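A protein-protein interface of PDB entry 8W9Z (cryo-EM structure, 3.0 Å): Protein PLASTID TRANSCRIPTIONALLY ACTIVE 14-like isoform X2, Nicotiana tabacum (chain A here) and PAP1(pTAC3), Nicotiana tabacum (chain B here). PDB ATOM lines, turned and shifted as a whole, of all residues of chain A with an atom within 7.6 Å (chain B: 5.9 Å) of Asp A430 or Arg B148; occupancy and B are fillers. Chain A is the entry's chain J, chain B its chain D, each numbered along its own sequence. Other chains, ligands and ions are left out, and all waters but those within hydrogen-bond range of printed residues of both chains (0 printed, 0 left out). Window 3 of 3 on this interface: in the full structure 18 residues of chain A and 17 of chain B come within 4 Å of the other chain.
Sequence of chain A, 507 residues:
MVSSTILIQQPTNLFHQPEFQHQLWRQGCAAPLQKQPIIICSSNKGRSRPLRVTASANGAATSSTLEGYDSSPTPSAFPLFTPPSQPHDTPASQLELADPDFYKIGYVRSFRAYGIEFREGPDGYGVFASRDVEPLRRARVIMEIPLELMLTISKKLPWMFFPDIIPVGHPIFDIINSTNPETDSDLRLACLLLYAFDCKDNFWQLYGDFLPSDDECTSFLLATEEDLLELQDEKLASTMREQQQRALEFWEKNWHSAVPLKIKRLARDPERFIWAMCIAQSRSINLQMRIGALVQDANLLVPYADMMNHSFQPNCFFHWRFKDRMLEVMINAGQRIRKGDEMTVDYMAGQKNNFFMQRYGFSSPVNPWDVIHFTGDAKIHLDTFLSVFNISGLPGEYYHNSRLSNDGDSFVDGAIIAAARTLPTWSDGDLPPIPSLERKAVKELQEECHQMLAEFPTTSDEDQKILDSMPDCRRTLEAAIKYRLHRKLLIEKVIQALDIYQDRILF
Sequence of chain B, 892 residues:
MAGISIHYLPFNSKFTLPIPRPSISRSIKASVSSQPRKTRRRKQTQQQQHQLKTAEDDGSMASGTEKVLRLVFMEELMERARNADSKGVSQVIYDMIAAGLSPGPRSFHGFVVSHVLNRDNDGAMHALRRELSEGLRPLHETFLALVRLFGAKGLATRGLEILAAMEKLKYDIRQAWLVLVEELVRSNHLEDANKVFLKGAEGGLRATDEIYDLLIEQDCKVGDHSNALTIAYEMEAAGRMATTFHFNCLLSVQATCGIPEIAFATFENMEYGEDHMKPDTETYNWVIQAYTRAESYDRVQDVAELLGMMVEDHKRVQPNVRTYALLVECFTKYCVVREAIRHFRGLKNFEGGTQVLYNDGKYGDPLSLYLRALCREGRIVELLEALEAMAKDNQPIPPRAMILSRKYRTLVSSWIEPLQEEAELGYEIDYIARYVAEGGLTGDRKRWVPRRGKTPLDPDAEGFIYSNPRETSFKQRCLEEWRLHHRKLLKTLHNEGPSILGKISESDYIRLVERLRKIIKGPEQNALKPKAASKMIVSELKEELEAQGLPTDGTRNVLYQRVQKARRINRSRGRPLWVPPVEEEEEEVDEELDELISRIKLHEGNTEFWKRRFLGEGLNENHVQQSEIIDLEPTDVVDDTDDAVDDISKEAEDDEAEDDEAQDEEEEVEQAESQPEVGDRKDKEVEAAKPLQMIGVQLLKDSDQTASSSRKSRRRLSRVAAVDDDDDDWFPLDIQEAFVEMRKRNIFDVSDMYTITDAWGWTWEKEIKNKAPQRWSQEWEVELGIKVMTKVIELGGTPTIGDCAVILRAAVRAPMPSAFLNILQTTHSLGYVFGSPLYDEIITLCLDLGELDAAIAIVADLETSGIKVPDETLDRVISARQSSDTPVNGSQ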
ATOM      1  N   HIS A 381       6.896  27.691  11.266  1.00  0.00           N
ATOM      2  CA  HIS A 381       8.171  27.052  10.972  1.00  0.00           C
ATOM      3  C   HIS A 381       8.105  25.570  11.317  1.00  0.00           C
ATOM      4  O   HIS A 381       7.563  25.184  12.356  1.00  0.00           O
ATOM      5  CB  HIS A 381       9.303  27.724  11.746  1.00  0.00           C
ATOM      6  CG  HIS A 381      10.666  27.408  11.216  1.00  0.00           C
ATOM      7  ND1 HIS A 381      11.163  27.970  10.060  1.00  0.00           N
ATOM      8  CD2 HIS A 381      11.635  26.585  11.681  1.00  0.00           C
ATOM      9  CE1 HIS A 381      12.380  27.509   9.836  1.00  0.00           C
ATOM     10  NE2 HIS A 381      12.691  26.668  10.805  1.00  0.00           N
ATOM     11  N   ASP A 383      10.885  23.054  11.218  1.00  0.00           N
ATOM     12  CA  ASP A 383      11.979  22.407  11.934  1.00  0.00           C
ATOM     13  C   ASP A 383      11.957  22.762  13.415  1.00  0.00           C
ATOM     14  O   ASP A 383      12.180  21.895  14.269  1.00  0.00           O
ATOM     15  CB  ASP A 383      13.318  22.787  11.302  1.00  0.00           C
ATOM     16  CG  ASP A 383      14.404  21.767  11.586  1.00  0.00           C
ATOM     17  OD1 ASP A 383      14.610  21.422  12.768  1.00  0.00           O
ATOM     18  OD2 ASP A 383      15.044  21.299  10.620  1.00  0.00           O
ATOM     19  N   SER A 427      10.004  26.476   5.048  1.00  0.00           N
ATOM     20  CA  SER A 427      11.399  26.226   5.397  1.00  0.00           C
ATOM     21  C   SER A 427      12.270  26.665   4.231  1.00  0.00           C
ATOM     22  O   SER A 427      12.123  26.150   3.119  1.00  0.00           O
ATOM     23  CB  SER A 427      11.633  24.750   5.722  1.00  0.00           C
ATOM     24  OG  SER A 427      12.964  24.527   6.150  1.00  0.00           O
ATOM     25  N   ASP A 428      13.167  27.614   4.484  1.00  0.00           N
ATOM     26  CA  ASP A 428      14.067  28.158   3.470  1.00  0.00           C
ATOM     27  C   ASP A 428      15.496  27.968   3.968  1.00  0.00           C
ATOM     28  O   ASP A 428      16.076  28.868   4.582  1.00  0.00           O
ATOM     29  CB  ASP A 428      13.752  29.632   3.191  1.00  0.00           C
ATOM     30  CG  ASP A 428      14.375  30.132   1.899  1.00  0.00           C
ATOM     31  OD1 ASP A 428      15.418  29.588   1.480  1.00  0.00           O
ATOM     32  OD2 ASP A 428      13.817  31.076   1.300  1.00  0.00           O
ATOM     33  N   GLY A 429      16.063  26.796   3.695  1.00  0.00           N
ATOM     34  CA  GLY A 429      17.432  26.529   4.099  1.00  0.00           C
ATOM     35  C   GLY A 429      17.576  26.493   5.607  1.00  0.00           C
ATOM     36  O   GLY A 429      16.754  25.911   6.324  1.00  0.00           O
ATOM     37  N   ASP A 430      18.639  27.127   6.100  1.00  0.00           N
ATOM     38  CA  ASP A 430      18.938  27.178   7.524  1.00  0.00           C
ATOM     39  C   ASP A 430      18.635  28.542   8.136  1.00  0.00           C
ATOM     40  O   ASP A 430      19.180  28.872   9.193  1.00  0.00           O
ATOM     41  CB  ASP A 430      20.402  26.807   7.768  1.00  0.00           C
ATOM     42  CG  ASP A 430      20.745  25.425   7.251  1.00  0.00           C
ATOM     43  OD1 ASP A 430      19.849  24.555   7.237  1.00  0.00           O
ATOM     44  OD2 ASP A 430      21.911  25.207   6.858  1.00  0.00           O
ATOM     45  N   LEU A 431      17.781  29.333   7.497  1.00  0.00           N
ATOM     46  CA  LEU A 431      17.468  30.659   8.010  1.00  0.00           C
ATOM     47  C   LEU A 431      16.753  30.545   9.353  1.00  0.00           C
ATOM     48  O   LEU A 431      15.749  29.826   9.457  1.00  0.00           O
ATOM     49  CB  LEU A 431      16.605  31.426   7.009  1.00  0.00           C
ATOM     50  CG  LEU A 431      16.168  32.841   7.395  1.00  0.00           C
ATOM     51  CD1 LEU A 431      16.354  33.790   6.222  1.00  0.00           C
ATOM     52  CD2 LEU A 431      14.720  32.850   7.856  1.00  0.00           C
ATOM     53  N   PRO A 432      17.228  31.227  10.397  1.00  0.00           N
ATOM     54  CA  PRO A 432      16.585  31.100  11.701  1.00  0.00           C
ATOM     55  C   PRO A 432      15.264  31.844  11.726  1.00  0.00           C
ATOM     56  O   PRO A 432      15.119  32.903  11.090  1.00  0.00           O
ATOM     57  CB  PRO A 432      17.606  31.734  12.660  1.00  0.00           C
ATOM     58  CG  PRO A 432      18.324  32.727  11.816  1.00  0.00           C
ATOM     59  CD  PRO A 432      18.398  32.122  10.437  1.00  0.00           C
ATOM     60  N   PRO A 433      14.271  31.334  12.448  1.00  0.00           N
ATOM     61  CA  PRO A 433      12.965  31.995  12.480  1.00  0.00           C
ATOM     62  C   PRO A 433      12.975  33.237  13.356  1.00  0.00           C
ATOM     63  O   PRO A 433      13.753  33.358  14.306  1.00  0.00           O
ATOM     64  CB  PRO A 433      12.046  30.918  13.067  1.00  0.00           C
ATOM     65  CG  PRO A 433      12.948  30.117  13.944  1.00  0.00           C
ATOM     66  CD  PRO A 433      14.292  30.103  13.257  1.00  0.00           C
ATOM     67  N   HIS B 109      21.579  28.989  18.870  1.00  0.00           N
ATOM     68  CA  HIS B 109      21.292  28.613  17.489  1.00  0.00           C
ATOM     69  C   HIS B 109      21.556  29.773  16.539  1.00  0.00           C
ATOM     70  O   HIS B 109      22.112  29.582  15.451  1.00  0.00           O
ATOM     71  CB  HIS B 109      19.846  28.134  17.364  1.00  0.00           C
ATOM     72  CG  HIS B 109      19.383  27.985  15.949  1.00  0.00           C
ATOM     73  ND1 HIS B 109      20.071  27.242  15.015  1.00  0.00           N
ATOM     74  CD2 HIS B 109      18.302  28.489  15.307  1.00  0.00           C
ATOM     75  CE1 HIS B 109      19.435  27.294  13.859  1.00  0.00           C
ATOM     76  NE2 HIS B 109      18.358  28.042  14.009  1.00  0.00           N
ATOM     77  N   VAL B 113      24.247  29.881  13.502  1.00  0.00           N
ATOM     78  CA  VAL B 113      23.829  30.111  12.125  1.00  0.00           C
ATOM     79  C   VAL B 113      24.437  31.387  11.556  1.00  0.00           C
ATOM     80  O   VAL B 113      24.564  31.512  10.333  1.00  0.00           O
ATOM     81  CB  VAL B 113      22.291  30.139  12.020  1.00  0.00           C
ATOM     82  CG1 VAL B 113      21.734  31.456  12.530  1.00  0.00           C
ATOM     83  CG2 VAL B 113      21.853  29.883  10.588  1.00  0.00           C
ATOM     84  N   VAL B 116      27.459  30.016  10.221  1.00  0.00           N
ATOM     85  CA  VAL B 116      27.138  29.066   9.159  1.00  0.00           C
ATOM     86  C   VAL B 116      26.823  29.795   7.858  1.00  0.00           C
ATOM     87  O   VAL B 116      27.262  29.381   6.778  1.00  0.00           O
ATOM     88  CB  VAL B 116      25.980  28.149   9.595  1.00  0.00           C
ATOM     89  CG1 VAL B 116      25.436  27.373   8.406  1.00  0.00           C
ATOM     90  CG2 VAL B 116      26.446  27.191  10.678  1.00  0.00           C
ATOM     91  N   LEU B 117      26.069  30.894   7.936  1.00  0.00           N
ATOM     92  CA  LEU B 117      25.710  31.625   6.724  1.00  0.00           C
ATOM     93  C   LEU B 117      26.918  32.304   6.092  1.00  0.00           C
ATOM     94  O   LEU B 117      26.918  32.561   4.883  1.00  0.00           O
ATOM     95  CB  LEU B 117      24.625  32.657   7.032  1.00  0.00           C
ATOM     96  CG  LEU B 117      23.240  32.108   7.375  1.00  0.00           C
ATOM     97  CD1 LEU B 117      22.266  33.243   7.644  1.00  0.00           C
ATOM     98  CD2 LEU B 117      22.728  31.212   6.259  1.00  0.00           C
ATOM     99  N   GLU B 141      18.708  21.267  14.879  1.00  0.00           N
ATOM    100  CA  GLU B 141      18.924  22.149  13.735  1.00  0.00           C
ATOM    101  C   GLU B 141      20.356  22.667  13.696  1.00  0.00           C
ATOM    102  O   GLU B 141      20.939  22.815  12.615  1.00  0.00           O
ATOM    103  CB  GLU B 141      17.925  23.306  13.772  1.00  0.00           C
ATOM    104  CG  GLU B 141      18.155  24.374  12.713  1.00  0.00           C
ATOM    105  CD  GLU B 141      18.011  23.852  11.296  1.00  0.00           C
ATOM    106  OE1 GLU B 141      17.305  22.842  11.098  1.00  0.00           O
ATOM    107  OE2 GLU B 141      18.604  24.456  10.377  1.00  0.00           O
ATOM    108  N   PHE B 143      23.100  21.086  14.826  1.00  0.00           N
ATOM    109  CA  PHE B 143      23.933  19.993  14.335  1.00  0.00           C
ATOM    110  C   PHE B 143      23.708  19.752  12.849  1.00  0.00           C
ATOM    111  O   PHE B 143      24.652  19.440  12.113  1.00  0.00           O
ATOM    112  CB  PHE B 143      23.657  18.723  15.138  1.00  0.00           C
ATOM    113  CG  PHE B 143      24.422  18.645  16.426  1.00  0.00           C
ATOM    114  CD1 PHE B 143      25.716  19.126  16.506  1.00  0.00           C
ATOM    115  CD2 PHE B 143      23.848  18.092  17.556  1.00  0.00           C
ATOM    116  CE1 PHE B 143      26.425  19.055  17.688  1.00  0.00           C
ATOM    117  CE2 PHE B 143      24.551  18.018  18.742  1.00  0.00           C
ATOM    118  CZ  PHE B 143      25.840  18.501  18.808  1.00  0.00           C
ATOM    119  N   LEU B 144      22.465  19.897  12.384  1.00  0.00           N
ATOM    120  CA  LEU B 144      22.188  19.726  10.963  1.00  0.00           C
ATOM    121  C   LEU B 144      22.895  20.791  10.135  1.00  0.00           C
ATOM    122  O   LEU B 144      23.471  20.490   9.082  1.00  0.00           O
ATOM    123  CB  LEU B 144      20.680  19.765  10.715  1.00  0.00           C
ATOM    124  CG  LEU B 144      20.212  19.432   9.299  1.00  0.00           C
ATOM    125  CD1 LEU B 144      20.595  18.007   8.934  1.00  0.00           C
ATOM    126  CD2 LEU B 144      18.712  19.638   9.166  1.00  0.00           C
ATOM    127  N   ALA B 145      22.869  22.042  10.600  1.00  0.00           N
ATOM    128  CA  ALA B 145      23.566  23.111   9.892  1.00  0.00           C
ATOM    129  C   ALA B 145      25.073  22.888   9.904  1.00  0.00           C
ATOM    130  O   ALA B 145      25.750  23.144   8.901  1.00  0.00           O
ATOM    131  CB  ALA B 145      23.216  24.464  10.508  1.00  0.00           C
ATOM    132  N   LEU B 146      25.614  22.405  11.024  1.00  0.00           N
ATOM    133  CA  LEU B 146      27.044  22.111  11.083  1.00  0.00           C
ATOM    134  C   LEU B 146      27.420  21.006  10.103  1.00  0.00           C
ATOM    135  O   LEU B 146      28.442  21.100   9.410  1.00  0.00           O
ATOM    136  CB  LEU B 146      27.445  21.722  12.505  1.00  0.00           C
ATOM    137  CG  LEU B 146      27.327  22.809  13.572  1.00  0.00           C
ATOM    138  CD1 LEU B 146      27.799  22.292  14.922  1.00  0.00           C
ATOM    139  CD2 LEU B 146      28.107  24.044  13.165  1.00  0.00           C
ATOM    140  N   VAL B 147      26.606  19.951  10.032  1.00  0.00           N
ATOM    141  CA  VAL B 147      26.878  18.858   9.102  1.00  0.00           C
ATOM    142  C   VAL B 147      26.790  19.349   7.662  1.00  0.00           C
ATOM    143  O   VAL B 147      27.618  18.988   6.816  1.00  0.00           O
ATOM    144  CB  VAL B 147      25.916  17.685   9.364  1.00  0.00           C
ATOM    145  CG1 VAL B 147      25.997  16.669   8.242  1.00  0.00           C
ATOM    146  CG2 VAL B 147      26.239  17.027  10.694  1.00  0.00           C
ATOM    147  N   ARG B 148      25.799  20.193   7.364  1.00  0.00           N
ATOM    148  CA  ARG B 148      25.671  20.732   6.015  1.00  0.00           C
ATOM    149  C   ARG B 148      26.869  21.598   5.648  1.00  0.00           C
ATOM    150  O   ARG B 148      27.376  21.526   4.522  1.00  0.00           O
ATOM    151  CB  ARG B 148      24.372  21.528   5.891  1.00  0.00           C
ATOM    152  CG  ARG B 148      24.151  22.150   4.524  1.00  0.00           C
ATOM    153  CD  ARG B 148      22.793  22.830   4.428  1.00  0.00           C
ATOM    154  NE  ARG B 148      21.689  21.876   4.487  1.00  0.00           N
ATOM    155  CZ  ARG B 148      20.964  21.634   5.574  1.00  0.00           C
ATOM    156  NH1 ARG B 148      21.223  22.278   6.703  1.00  0.00           N
ATOM    157  NH2 ARG B 148      19.980  20.748   5.532  1.00  0.00           N
ATOM    158  N   LEU B 149      27.342  22.419   6.589  1.00  0.00           N
ATOM    159  CA  LEU B 149      28.492  23.272   6.313  1.00  0.00           C
ATOM    160  C   LEU B 149      29.758  22.450   6.117  1.00  0.00           C
ATOM    161  O   LEU B 149      30.572  22.753   5.237  1.00  0.00           O
ATOM    162  CB  LEU B 149      28.677  24.288   7.441  1.00  0.00           C
ATOM    163  CG  LEU B 149      29.860  25.248   7.307  1.00  0.00           C
ATOM    164  CD1 LEU B 149      29.421  26.677   7.575  1.00  0.00           C
ATOM    165  CD2 LEU B 149      30.984  24.852   8.250  1.00  0.00           C
ATOM    166  N   PHE B 150      29.945  21.403   6.925  1.00  0.00           N
ATOM    167  CA  PHE B 150      31.122  20.556   6.761  1.00  0.00           C
ATOM    168  C   PHE B 150      31.061  19.751   5.470  1.00  0.00           C
ATOM    169  O   PHE B 150      32.104  19.458   4.875  1.00  0.00           O
ATOM    170  CB  PHE B 150      31.277  19.625   7.962  1.00  0.00           C
ATOM    171  CG  PHE B 150      31.638  20.334   9.233  1.00  0.00           C
ATOM    172  CD1 PHE B 150      32.209  21.595   9.199  1.00  0.00           C
ATOM    173  CD2 PHE B 150      31.410  19.742  10.463  1.00  0.00           C
ATOM    174  CE1 PHE B 150      32.543  22.252  10.365  1.00  0.00           C
ATOM    175  CE2 PHE B 150      31.742  20.395  11.632  1.00  0.00           C
ATOM    176  CZ  PHE B 150      32.310  21.651  11.583  1.00  0.00           C
ATOM    177  N   GLY B 151      29.858  19.384   5.022  1.00  0.00           N
ATOM    178  CA  GLY B 151      29.734  18.671   3.765  1.00  0.00           C
ATOM    179  C   GLY B 151      29.903  19.553   2.549  1.00  0.00           C
ATOM    180  O   GLY B 151      30.409  19.097   1.519  1.00  0.00           O
ATOM    181  N   ALA B 152      29.486  20.817   2.640  1.00  0.00           N
ATOM    182  CA  ALA B 152      29.647  21.727   1.511  1.00  0.00           C
ATOM    183  C   ALA B 152      31.115  22.061   1.278  1.00  0.00           C
ATOM    184  O   ALA B 152      31.545  22.227   0.131  1.00  0.00           O
ATOM    185  CB  ALA B 152      28.835  23.000   1.741  1.00  0.00           C
ATOM    186  N   LYS B 153      31.897  22.162   2.350  1.00  0.00           N
ATOM    187  CA  LYS B 153      33.317  22.471   2.250  1.00  0.00           C
ATOM    188  C   LYS B 153      34.165  21.263   1.880  1.00  0.00           C
ATOM    189  O   LYS B 153      35.382  21.409   1.719  1.00  0.00           O
ATOM    190  CB  LYS B 153      33.821  23.062   3.569  1.00  0.00           C
ATOM    191  CG  LYS B 153      33.245  24.427   3.902  1.00  0.00           C
ATOM    192  CD  LYS B 153      33.670  25.466   2.880  1.00  0.00           C
ATOM    193  CE  LYS B 153      33.154  26.845   3.249  1.00  0.00           C
ATOM    194  NZ  LYS B 153      33.586  27.879   2.269  1.00  0.00           N
ATOM    195  N   VAL B 179      21.816  14.246   4.701  1.00  0.00           N
ATOM    196  CA  VAL B 179      22.219  15.597   4.320  1.00  0.00           C
ATOM    197  C   VAL B 179      23.717  15.647   4.059  1.00  0.00           C
ATOM    198  O   VAL B 179      24.178  16.302   3.116  1.00  0.00           O
ATOM    199  CB  VAL B 179      21.793  16.609   5.399  1.00  0.00           C
ATOM    200  CG1 VAL B 179      22.391  17.977   5.115  1.00  0.00           C
ATOM    201  CG2 VAL B 179      20.277  16.703   5.465  1.00  0.00           C
ATOM    202  N   GLU B 183      25.220  16.665   0.427  1.00  0.00           N
ATOM    203  CA  GLU B 183      26.070  17.841   0.277  1.00  0.00           C
ATOM    204  C   GLU B 183      27.470  17.468  -0.192  1.00  0.00           C
ATOM    205  O   GLU B 183      28.116  18.259  -0.888  1.00  0.00           O
ATOM    206  CB  GLU B 183      26.134  18.619   1.590  1.00  0.00           C
ATOM    207  CG  GLU B 183      24.816  19.266   1.988  1.00  0.00           C
ATOM    208  CD  GLU B 183      24.336  20.289   0.975  1.00  0.00           C
ATOM    209  OE1 GLU B 183      25.187  20.930   0.322  1.00  0.00           O
ATOM    210  OE2 GLU B 183      23.107  20.450   0.832  1.00  0.00           O
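OD1 of Asp A430 sits close to OE2 of Glu B141 (3.4 Å).
The side-chain carboxylate (OD2) of Asp A383 sits close to the side-chain carboxylate (OE1) of Glu B141.
OD1 of Asp A430 lies within salt-bridge range of NH1 of Arg B148 (2.7 Å).
Among the printed residues, pairs that only touch across the chains: Asp A430 with Val B113, Pro A432 with Val B113 and Asp A430 with Ala B145.
Of the printed residues of chain B, Asp A383 touches Glu B141.
Printed residues of chain A within 4 Å of Glu B141: Asp A383 and Asp A430.
The nearest printed residue of chain A that does not touch Glu B141 is Gly A429 (4.7 Å).
Hydrophobic or aromatic side chains of chain B within 4 Å of the printed part of chain A: Val B113 and Ala B145.
Of the 9 printed residues of chain A, 3 touch a printed residue of chain B.
Hydrophobic or aromatic side chains of chain A within 4 Å of the printed part of chain B: Pro A432.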
